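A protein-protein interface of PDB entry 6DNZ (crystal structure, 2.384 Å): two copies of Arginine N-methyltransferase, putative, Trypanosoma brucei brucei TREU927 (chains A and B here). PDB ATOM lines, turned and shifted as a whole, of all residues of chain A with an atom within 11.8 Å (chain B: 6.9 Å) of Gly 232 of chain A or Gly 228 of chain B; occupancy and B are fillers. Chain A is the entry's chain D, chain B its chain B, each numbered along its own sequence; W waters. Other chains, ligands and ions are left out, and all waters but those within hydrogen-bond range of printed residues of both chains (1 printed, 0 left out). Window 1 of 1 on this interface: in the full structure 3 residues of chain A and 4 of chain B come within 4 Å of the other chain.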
ATOM      1  N   GLU A 225     -17.296  28.940 -30.266  1.00  0.00           N
ATOM      2  CA  GLU A 225     -16.318  29.013 -29.195  1.00  0.00           C
ATOM      3  C   GLU A 225     -16.278  27.737 -28.369  1.00  0.00           C
ATOM      4  O   GLU A 225     -15.280  27.494 -27.687  1.00  0.00           O
ATOM      5  CB  GLU A 225     -16.600  30.210 -28.289  1.00  0.00           C
ATOM      6  CG  GLU A 225     -15.343  30.812 -27.668  1.00  0.00           C
ATOM      7  CD  GLU A 225     -14.347  31.276 -28.716  1.00  0.00           C
ATOM      8  OE1 GLU A 225     -14.780  31.814 -29.757  1.00  0.00           O
ATOM      9  OE2 GLU A 225     -13.134  31.081 -28.503  1.00  0.00           O
ATOM     10  N   PHE A 226     -17.335  26.925 -28.414  1.00  0.00           N
ATOM     11  CA  PHE A 226     -17.322  25.645 -27.716  1.00  0.00           C
ATOM     12  C   PHE A 226     -16.099  24.824 -28.097  1.00  0.00           C
ATOM     13  O   PHE A 226     -15.489  24.167 -27.245  1.00  0.00           O
ATOM     14  CB  PHE A 226     -18.607  24.876 -28.031  1.00  0.00           C
ATOM     15  CG  PHE A 226     -18.505  23.398 -27.792  1.00  0.00           C
ATOM     16  CD1 PHE A 226     -18.709  22.872 -26.530  1.00  0.00           C
ATOM     17  CD2 PHE A 226     -18.219  22.532 -28.835  1.00  0.00           C
ATOM     18  CE1 PHE A 226     -18.621  21.513 -26.310  1.00  0.00           C
ATOM     19  CE2 PHE A 226     -18.130  21.174 -28.619  1.00  0.00           C
ATOM     20  CZ  PHE A 226     -18.332  20.664 -27.356  1.00  0.00           C
ATOM     21  N   TRP A 227     -15.724  24.850 -29.375  1.00  0.00           N
ATOM     22  CA  TRP A 227     -14.569  24.096 -29.840  1.00  0.00           C
ATOM     23  C   TRP A 227     -13.255  24.701 -29.375  1.00  0.00           C
ATOM     24  O   TRP A 227     -12.205  24.076 -29.562  1.00  0.00           O
ATOM     25  CB  TRP A 227     -14.586  24.010 -31.366  1.00  0.00           C
ATOM     26  CG  TRP A 227     -15.914  23.596 -31.905  1.00  0.00           C
ATOM     27  CD1 TRP A 227     -16.903  24.415 -32.351  1.00  0.00           C
ATOM     28  CD2 TRP A 227     -16.407  22.259 -32.042  1.00  0.00           C
ATOM     29  NE1 TRP A 227     -17.982  23.673 -32.763  1.00  0.00           N
ATOM     30  CE2 TRP A 227     -17.701  22.345 -32.584  1.00  0.00           C
ATOM     31  CE3 TRP A 227     -15.879  20.999 -31.762  1.00  0.00           C
ATOM     32  CZ2 TRP A 227     -18.474  21.222 -32.852  1.00  0.00           C
ATOM     33  CZ3 TRP A 227     -16.649  19.883 -32.031  1.00  0.00           C
ATOM     34  CH2 TRP A 227     -17.931  20.002 -32.569  1.00  0.00           C
ATOM     35  N   GLY A 228     -13.286  25.895 -28.783  1.00  0.00           N
ATOM     36  CA  GLY A 228     -12.065  26.482 -28.265  1.00  0.00           C
ATOM     37  C   GLY A 228     -11.329  25.545 -27.332  1.00  0.00           C
ATOM     38  O   GLY A 228     -10.098  25.486 -27.335  1.00  0.00           O
ATOM     39  N   ASN A 229     -12.073  24.791 -26.525  1.00  0.00           N
ATOM     40  CA  ASN A 229     -11.448  23.794 -25.662  1.00  0.00           C
ATOM     41  C   ASN A 229     -12.479  22.756 -25.256  1.00  0.00           C
ATOM     42  O   ASN A 229     -13.488  23.094 -24.629  1.00  0.00           O
ATOM     43  CB  ASN A 229     -10.834  24.447 -24.440  1.00  0.00           C
ATOM     44  CG  ASN A 229      -9.609  23.712 -23.961  1.00  0.00           C
ATOM     45  OD1 ASN A 229      -9.715  22.652 -23.346  1.00  0.00           O
ATOM     46  ND2 ASN A 229      -8.435  24.271 -24.233  1.00  0.00           N
ATOM     47  N   VAL A 230     -12.207  21.497 -25.584  1.00  0.00           N
ATOM     48  CA  VAL A 230     -13.142  20.395 -25.387  1.00  0.00           C
ATOM     49  C   VAL A 230     -12.442  19.382 -24.489  1.00  0.00           C
ATOM     50  O   VAL A 230     -11.563  18.639 -24.940  1.00  0.00           O
ATOM     51  CB  VAL A 230     -13.575  19.773 -26.719  1.00  0.00           C
ATOM     52  CG1 VAL A 230     -14.456  18.562 -26.493  1.00  0.00           C
ATOM     53  CG2 VAL A 230     -14.300  20.806 -27.570  1.00  0.00           C
ATOM     54  N   TYR A 231     -12.819  19.357 -23.210  1.00  0.00           N
ATOM     55  CA  TYR A 231     -12.220  18.447 -22.233  1.00  0.00           C
ATOM     56  C   TYR A 231     -10.707  18.633 -22.157  1.00  0.00           C
ATOM     57  O   TYR A 231      -9.946  17.665 -22.095  1.00  0.00           O
ATOM     58  CB  TYR A 231     -12.570  16.991 -22.548  1.00  0.00           C
ATOM     59  CG  TYR A 231     -14.052  16.715 -22.510  1.00  0.00           C
ATOM     60  CD1 TYR A 231     -14.662  16.247 -21.355  1.00  0.00           C
ATOM     61  CD2 TYR A 231     -14.842  16.934 -23.625  1.00  0.00           C
ATOM     62  CE1 TYR A 231     -16.017  16.001 -21.318  1.00  0.00           C
ATOM     63  CE2 TYR A 231     -16.195  16.693 -23.598  1.00  0.00           C
ATOM     64  CZ  TYR A 231     -16.778  16.228 -22.442  1.00  0.00           C
ATOM     65  OH  TYR A 231     -18.129  15.985 -22.417  1.00  0.00           O
ATOM     66  N   GLY A 232     -10.267  19.889 -22.159  1.00  0.00           N
ATOM     67  CA  GLY A 232      -8.862  20.209 -22.044  1.00  0.00           C
ATOM     68  C   GLY A 232      -8.122  20.358 -23.357  1.00  0.00           C
ATOM     69  O   GLY A 232      -6.987  20.852 -23.353  1.00  0.00           O
ATOM     70  N   PHE A 233      -8.726  19.970 -24.475  1.00  0.00           N
ATOM     71  CA  PHE A 233      -8.063  19.984 -25.770  1.00  0.00           C
ATOM     72  C   PHE A 233      -8.676  21.057 -26.656  1.00  0.00           C
ATOM     73  O   PHE A 233      -9.880  21.316 -26.592  1.00  0.00           O
ATOM     74  CB  PHE A 233      -8.177  18.622 -26.455  1.00  0.00           C
ATOM     75  CG  PHE A 233      -7.794  17.474 -25.573  1.00  0.00           C
ATOM     76  CD1 PHE A 233      -6.465  17.226 -25.279  1.00  0.00           C
ATOM     77  CD2 PHE A 233      -8.761  16.642 -25.040  1.00  0.00           C
ATOM     78  CE1 PHE A 233      -6.110  16.171 -24.467  1.00  0.00           C
ATOM     79  CE2 PHE A 233      -8.411  15.586 -24.230  1.00  0.00           C
ATOM     80  CZ  PHE A 233      -7.084  15.349 -23.942  1.00  0.00           C
ATOM     81  N   LYS A 234      -7.840  21.676 -27.486  1.00  0.00           N
ATOM     82  CA  LYS A 234      -8.287  22.715 -28.405  1.00  0.00           C
ATOM     83  C   LYS A 234      -8.681  22.081 -29.733  1.00  0.00           C
ATOM     84  O   LYS A 234      -7.858  21.421 -30.379  1.00  0.00           O
ATOM     85  CB  LYS A 234      -7.191  23.757 -28.614  1.00  0.00           C
ATOM     86  CG  LYS A 234      -6.781  24.487 -27.346  1.00  0.00           C
ATOM     87  CD  LYS A 234      -6.007  25.756 -27.661  1.00  0.00           C
ATOM     88  CE  LYS A 234      -5.547  26.458 -26.395  1.00  0.00           C
ATOM     89  NZ  LYS A 234      -4.933  27.788 -26.677  1.00  0.00           N
ATOM     90  N   MET A 235      -9.930  22.289 -30.140  1.00  0.00           N
ATOM     91  CA  MET A 235     -10.435  21.731 -31.388  1.00  0.00           C
ATOM     92  C   MET A 235     -10.747  22.850 -32.373  1.00  0.00           C
ATOM     93  O   MET A 235     -11.832  22.900 -32.947  1.00  0.00           O
ATOM     94  CB  MET A 235     -11.683  20.886 -31.139  1.00  0.00           C
ATOM     95  CG  MET A 235     -11.601  20.020 -29.899  1.00  0.00           C
ATOM     96  SD  MET A 235     -12.293  18.220 -30.170  1.00  0.00           S
ATOM     97  CE  MET A 235     -13.982  18.638 -30.994  1.00  0.00           C
ATOM     98  N   GLU A 236      -9.780  23.744 -32.556  1.00  0.00           N
ATOM     99  CA  GLU A 236      -9.951  24.862 -33.479  1.00  0.00           C
ATOM    100  C   GLU A 236     -10.437  24.439 -34.861  1.00  0.00           C
ATOM    101  O   GLU A 236     -11.337  25.106 -35.398  1.00  0.00           O
ATOM    102  CB  GLU A 236      -8.623  25.625 -33.596  1.00  0.00           C
ATOM    103  CG  GLU A 236      -8.767  27.074 -34.027  1.00  0.00           C
ATOM    104  CD  GLU A 236      -9.384  27.939 -32.945  1.00  0.00           C
ATOM    105  OE1 GLU A 236      -9.570  27.434 -31.818  1.00  0.00           O
ATOM    106  OE2 GLU A 236      -9.681  29.121 -33.218  1.00  0.00           O
ATOM    107  N   VAL B 224      -5.773  20.219 -10.467  1.00  0.00           N
ATOM    108  CA  VAL B 224      -4.665  20.028 -11.402  1.00  0.00           C
ATOM    109  C   VAL B 224      -5.150  20.102 -12.846  1.00  0.00           C
ATOM    110  O   VAL B 224      -4.735  20.980 -13.605  1.00  0.00           O
ATOM    111  CB  VAL B 224      -3.931  18.698 -11.125  1.00  0.00           C
ATOM    112  CG1 VAL B 224      -2.803  18.494 -12.125  1.00  0.00           C
ATOM    113  CG2 VAL B 224      -3.399  18.681  -9.704  1.00  0.00           C
ATOM    114  N   GLU B 225      -6.032  19.187 -13.247  1.00  0.00           N
ATOM    115  CA  GLU B 225      -6.549  19.217 -14.610  1.00  0.00           C
ATOM    116  C   GLU B 225      -7.388  20.456 -14.882  1.00  0.00           C
ATOM    117  O   GLU B 225      -7.565  20.822 -16.048  1.00  0.00           O
ATOM    118  CB  GLU B 225      -7.374  17.962 -14.890  1.00  0.00           C
ATOM    119  CG  GLU B 225      -6.611  16.870 -15.624  1.00  0.00           C
ATOM    120  CD  GLU B 225      -6.121  17.318 -16.988  1.00  0.00           C
ATOM    121  OE1 GLU B 225      -4.892  17.292 -17.215  1.00  0.00           O
ATOM    122  OE2 GLU B 225      -6.966  17.711 -17.825  1.00  0.00           O
ATOM    123  N   PHE B 226      -7.907  21.108 -13.840  1.00  0.00           N
ATOM    124  CA  PHE B 226      -8.628  22.360 -14.040  1.00  0.00           C
ATOM    125  C   PHE B 226      -7.805  23.345 -14.858  1.00  0.00           C
ATOM    126  O   PHE B 226      -8.346  24.075 -15.696  1.00  0.00           O
ATOM    127  CB  PHE B 226      -8.995  22.978 -12.693  1.00  0.00           C
ATOM    128  CG  PHE B 226      -9.306  24.445 -12.773  1.00  0.00           C
ATOM    129  CD1 PHE B 226     -10.566  24.882 -13.144  1.00  0.00           C
ATOM    130  CD2 PHE B 226      -8.337  25.389 -12.482  1.00  0.00           C
ATOM    131  CE1 PHE B 226     -10.854  26.230 -13.219  1.00  0.00           C
ATOM    132  CE2 PHE B 226      -8.621  26.739 -12.557  1.00  0.00           C
ATOM    133  CZ  PHE B 226      -9.880  27.159 -12.927  1.00  0.00           C
ATOM    134  N   TRP B 227      -6.492  23.385 -14.623  1.00  0.00           N
ATOM    135  CA  TRP B 227      -5.622  24.303 -15.346  1.00  0.00           C
ATOM    136  C   TRP B 227      -5.362  23.854 -16.773  1.00  0.00           C
ATOM    137  O   TRP B 227      -4.767  24.615 -17.544  1.00  0.00           O
ATOM    138  CB  TRP B 227      -4.290  24.457 -14.611  1.00  0.00           C
ATOM    139  CG  TRP B 227      -4.459  24.714 -13.157  1.00  0.00           C
ATOM    140  CD1 TRP B 227      -4.381  23.801 -12.155  1.00  0.00           C
ATOM    141  CD2 TRP B 227      -4.751  25.970 -12.536  1.00  0.00           C
ATOM    142  NE1 TRP B 227      -4.602  24.407 -10.943  1.00  0.00           N
ATOM    143  CE2 TRP B 227      -4.831  25.741 -11.151  1.00  0.00           C
ATOM    144  CE3 TRP B 227      -4.952  27.264 -13.016  1.00  0.00           C
ATOM    145  CZ2 TRP B 227      -5.100  26.759 -10.241  1.00  0.00           C
ATOM    146  CZ3 TRP B 227      -5.218  28.275 -12.110  1.00  0.00           C
ATOM    147  CH2 TRP B 227      -5.290  28.018 -10.741  1.00  0.00           C
ATOM    148  N   GLY B 228      -5.779  22.642 -17.138  1.00  0.00           N
ATOM    149  CA  GLY B 228      -5.646  22.211 -18.515  1.00  0.00           C
ATOM    150  C   GLY B 228      -6.350  23.135 -19.486  1.00  0.00           C
ATOM    151  O   GLY B 228      -5.920  23.281 -20.633  1.00  0.00           O
ATOM    152  N   ASN B 229      -7.430  23.777 -19.047  1.00  0.00           N
ATOM    153  CA  ASN B 229      -8.170  24.683 -19.921  1.00  0.00           C
ATOM    154  C   ASN B 229      -9.027  25.614 -19.084  1.00  0.00           C
ATOM    155  O   ASN B 229      -9.931  25.164 -18.373  1.00  0.00           O
ATOM    156  CB  ASN B 229      -9.014  23.886 -20.901  1.00  0.00           C
ATOM    157  CG  ASN B 229     -10.429  24.425 -21.046  1.00  0.00           C
ATOM    158  OD1 ASN B 229     -10.638  25.585 -21.402  1.00  0.00           O
ATOM    159  ND2 ASN B 229     -11.412  23.565 -20.799  1.00  0.00           N
ATOM    160  N   VAL B 230      -8.749  26.910 -19.182  1.00  0.00           N
ATOM    161  CA  VAL B 230      -9.429  27.935 -18.401  1.00  0.00           C
ATOM    162  C   VAL B 230     -10.019  28.917 -19.405  1.00  0.00           C
ATOM    163  O   VAL B 230      -9.308  29.771 -19.947  1.00  0.00           O
ATOM    164  CB  VAL B 230      -8.481  28.630 -17.418  1.00  0.00           C
ATOM    165  CG1 VAL B 230      -9.209  29.716 -16.646  1.00  0.00           C
ATOM    166  CG2 VAL B 230      -7.871  27.609 -16.466  1.00  0.00           C
ATOM    167  N   GLY B 232     -10.836  28.424 -22.375  1.00  0.00           N
ATOM    168  CA  GLY B 232     -10.251  28.215 -23.680  1.00  0.00           C
ATOM    169  C   GLY B 232      -8.739  28.272 -23.719  1.00  0.00           C
ATOM    170  O   GLY B 232      -8.156  27.986 -24.772  1.00  0.00           O
ATOM    171  N   PHE B 233      -8.091  28.623 -22.611  1.00  0.00           N
ATOM    172  CA  PHE B 233      -6.646  28.795 -22.563  1.00  0.00           C
ATOM    173  C   PHE B 233      -6.027  27.750 -21.646  1.00  0.00           C
ATOM    174  O   PHE B 233      -6.591  27.416 -20.599  1.00  0.00           O
ATOM    175  CB  PHE B 233      -6.279  30.200 -22.076  1.00  0.00           C
ATOM    176  CG  PHE B 233      -7.034  31.293 -22.771  1.00  0.00           C
ATOM    177  CD1 PHE B 233      -6.776  31.597 -24.097  1.00  0.00           C
ATOM    178  CD2 PHE B 233      -8.005  32.014 -22.101  1.00  0.00           C
ATOM    179  CE1 PHE B 233      -7.473  32.600 -24.741  1.00  0.00           C
ATOM    180  CE2 PHE B 233      -8.707  33.019 -22.738  1.00  0.00           C
ATOM    181  CZ  PHE B 233      -8.441  33.313 -24.059  1.00  0.00           C
ATOM    182  N   LYS B 234      -4.866  27.239 -22.046  1.00  0.00           N
ATOM    183  CA  LYS B 234      -4.146  26.251 -21.258  1.00  0.00           C
ATOM    184  C   LYS B 234      -3.268  26.961 -20.238  1.00  0.00           C
ATOM    185  O   LYS B 234      -2.528  27.886 -20.587  1.00  0.00           O
ATOM    186  CB  LYS B 234      -3.290  25.358 -22.156  1.00  0.00           C
ATOM    187  CG  LYS B 234      -4.082  24.619 -23.215  1.00  0.00           C
ATOM    188  CD  LYS B 234      -3.231  23.575 -23.921  1.00  0.00           C
ATOM    189  CE  LYS B 234      -4.011  22.882 -25.029  1.00  0.00           C
ATOM    190  NZ  LYS B 234      -3.288  21.698 -25.573  1.00  0.00           N
ATOM    191  N   MET B 235      -3.355  26.528 -18.985  1.00  0.00           N
ATOM    192  CA  MET B 235      -2.568  27.127 -17.915  1.00  0.00           C
ATOM    193  C   MET B 235      -1.712  26.056 -17.249  1.00  0.00           C
ATOM    194  O   MET B 235      -1.720  25.903 -16.028  1.00  0.00           O
ATOM    195  CB  MET B 235      -3.476  27.808 -16.886  1.00  0.00           C
ATOM    196  CG  MET B 235      -4.574  28.664 -17.504  1.00  0.00           C
ATOM    197  SD  MET B 235      -4.848  30.389 -16.628  1.00  0.00           S
ATOM    198  CE  MET B 235      -4.962  29.816 -14.794  1.00  0.00           C
ATOM    199  N   GLU B 236      -0.970  25.320 -18.073  1.00  0.00           N
ATOM    200  CA  GLU B 236      -0.127  24.241 -17.571  1.00  0.00           C
ATOM    201  C   GLU B 236       0.829  24.680 -16.469  1.00  0.00           C
ATOM    202  O   GLU B 236       0.986  23.926 -15.494  1.00  0.00           O
ATOM    203  CB  GLU B 236       0.657  23.632 -18.743  1.00  0.00           C
ATOM    204  CG  GLU B 236       1.166  22.226 -18.484  1.00  0.00           C
ATOM    205  CD  GLU B 236       0.051  21.197 -18.483  1.00  0.00           C
ATOM    206  OE1 GLU B 236      -1.078  21.543 -18.891  1.00  0.00           O
ATOM    207  OE2 GLU B 236       0.308  20.044 -18.078  1.00  0.00           O
ATOM    208  N   LYS B 239      -0.204  23.971 -12.811  1.00  0.00           N
ATOM    209  CA  LYS B 239      -0.230  22.614 -12.271  1.00  0.00           C
ATOM    210  C   LYS B 239       0.956  22.370 -11.349  1.00  0.00           C
ATOM    211  O   LYS B 239       0.803  21.794 -10.265  1.00  0.00           O
ATOM    212  CB  LYS B 239      -0.234  21.592 -13.407  1.00  0.00           C
ATOM    213  CG  LYS B 239      -1.440  21.685 -14.322  1.00  0.00           C
ATOM    214  CD  LYS B 239      -1.446  20.560 -15.343  1.00  0.00           C
ATOM    215  CE  LYS B 239      -2.599  20.704 -16.323  1.00  0.00           C
ATOM    216  NZ  LYS B 239      -2.674  19.568 -17.287  1.00  0.00           N
HETATM  217  O   HOH W   1      -6.889  17.703 -20.909  1.00  0.00           O
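OD1 of Asn 229 of chain A sits close to ND2 of Asn 229 of chain B (3.2 Å).
N of Gly 232 of chain B is in hydrogen-bond range of OD1 of Asn 229 of chain B.
The side-chain amide oxygen of Asn 229 of chain A lies close to the backbone NH of Gly 232 of chain A (3.1 Å).
N of Phe 233 of chain A is in hydrogen-bond range of OD1 of Asn 229 of chain A, 3.1 Å away.
Among the printed residues, merely in contact across the chains: Asn 229 of chain A with Gly 232 of chain B (3.8 Å), Gly 232 of chain A with Gly 228 of chain B (3.8 Å), Gly 232 of chain A with Asn 229 of chain B (3.9 Å), Gly 232 of chain A with Lys 234 of chain B (3.97 Å), Lys 234 of chain A with Gly 232 of chain B (3.4 Å) and Lys 234 of chain A with Lys 234 of chain B (3.95 Å).
Gly 232 of chain A touches three residues of chain B.
Gly 228 of chain B touches just one residue of chain A: Gly 232 (3.8 Å).
Val 230 of chain B touches none of the printed residues of chain A.
Of chain A, only Asn 229 and Lys 234 come within 4 Å of Gly 232 of chain B.
Lys 234 of chain B touches just these residues of chain A: Gly 232 and Lys 234.
Printed residues of chain B within 4 Å of Lys 234 of chain A: Gly 232 and Lys 234.
Of the printed residues of chain B, Asn 229 of chain A touches Asn 229 and Gly 232.
Glu 225 of chain A touches none of the printed residues of chain B.
The nearest printed residue of chain B that does not touch Asn 229 of chain A is Lys 234 of chain B (4.5 Å).
Along chain A the printed residues that touch a printed residue of chain B span positions 229 to 234.
Among the printed residues, no Asp or Glu carboxylate lies within 4 Å of a Lys or Arg side-chain nitrogen of the other chain.
Asn 229 of chain B touches its own counterpart, Asn 229 of chain A.
Asn 229 of chain A touches Gly 232 of chain B, and with the chains exchanged Gly 232 of chain A touches Asn 229 of chain B.
Gly 232 of chain A touches Gly 228 of chain B, but with the chains exchanged Gly 228 of chain A does not touch Gly 232 of chain B (4.1 Å).
Gly 232 of chain A touches Lys 234 of chain B, and with the chains exchanged Lys 234 of chain A touches Gly 232 of chain B.
Positions printed for both chains: 225, 226, 227, 228, 229, 230, 232, 233, 234, 235 and 236.
Water W1 bridges OE2 of Glu 225 of chain B and O of Tyr 231 of chain A.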
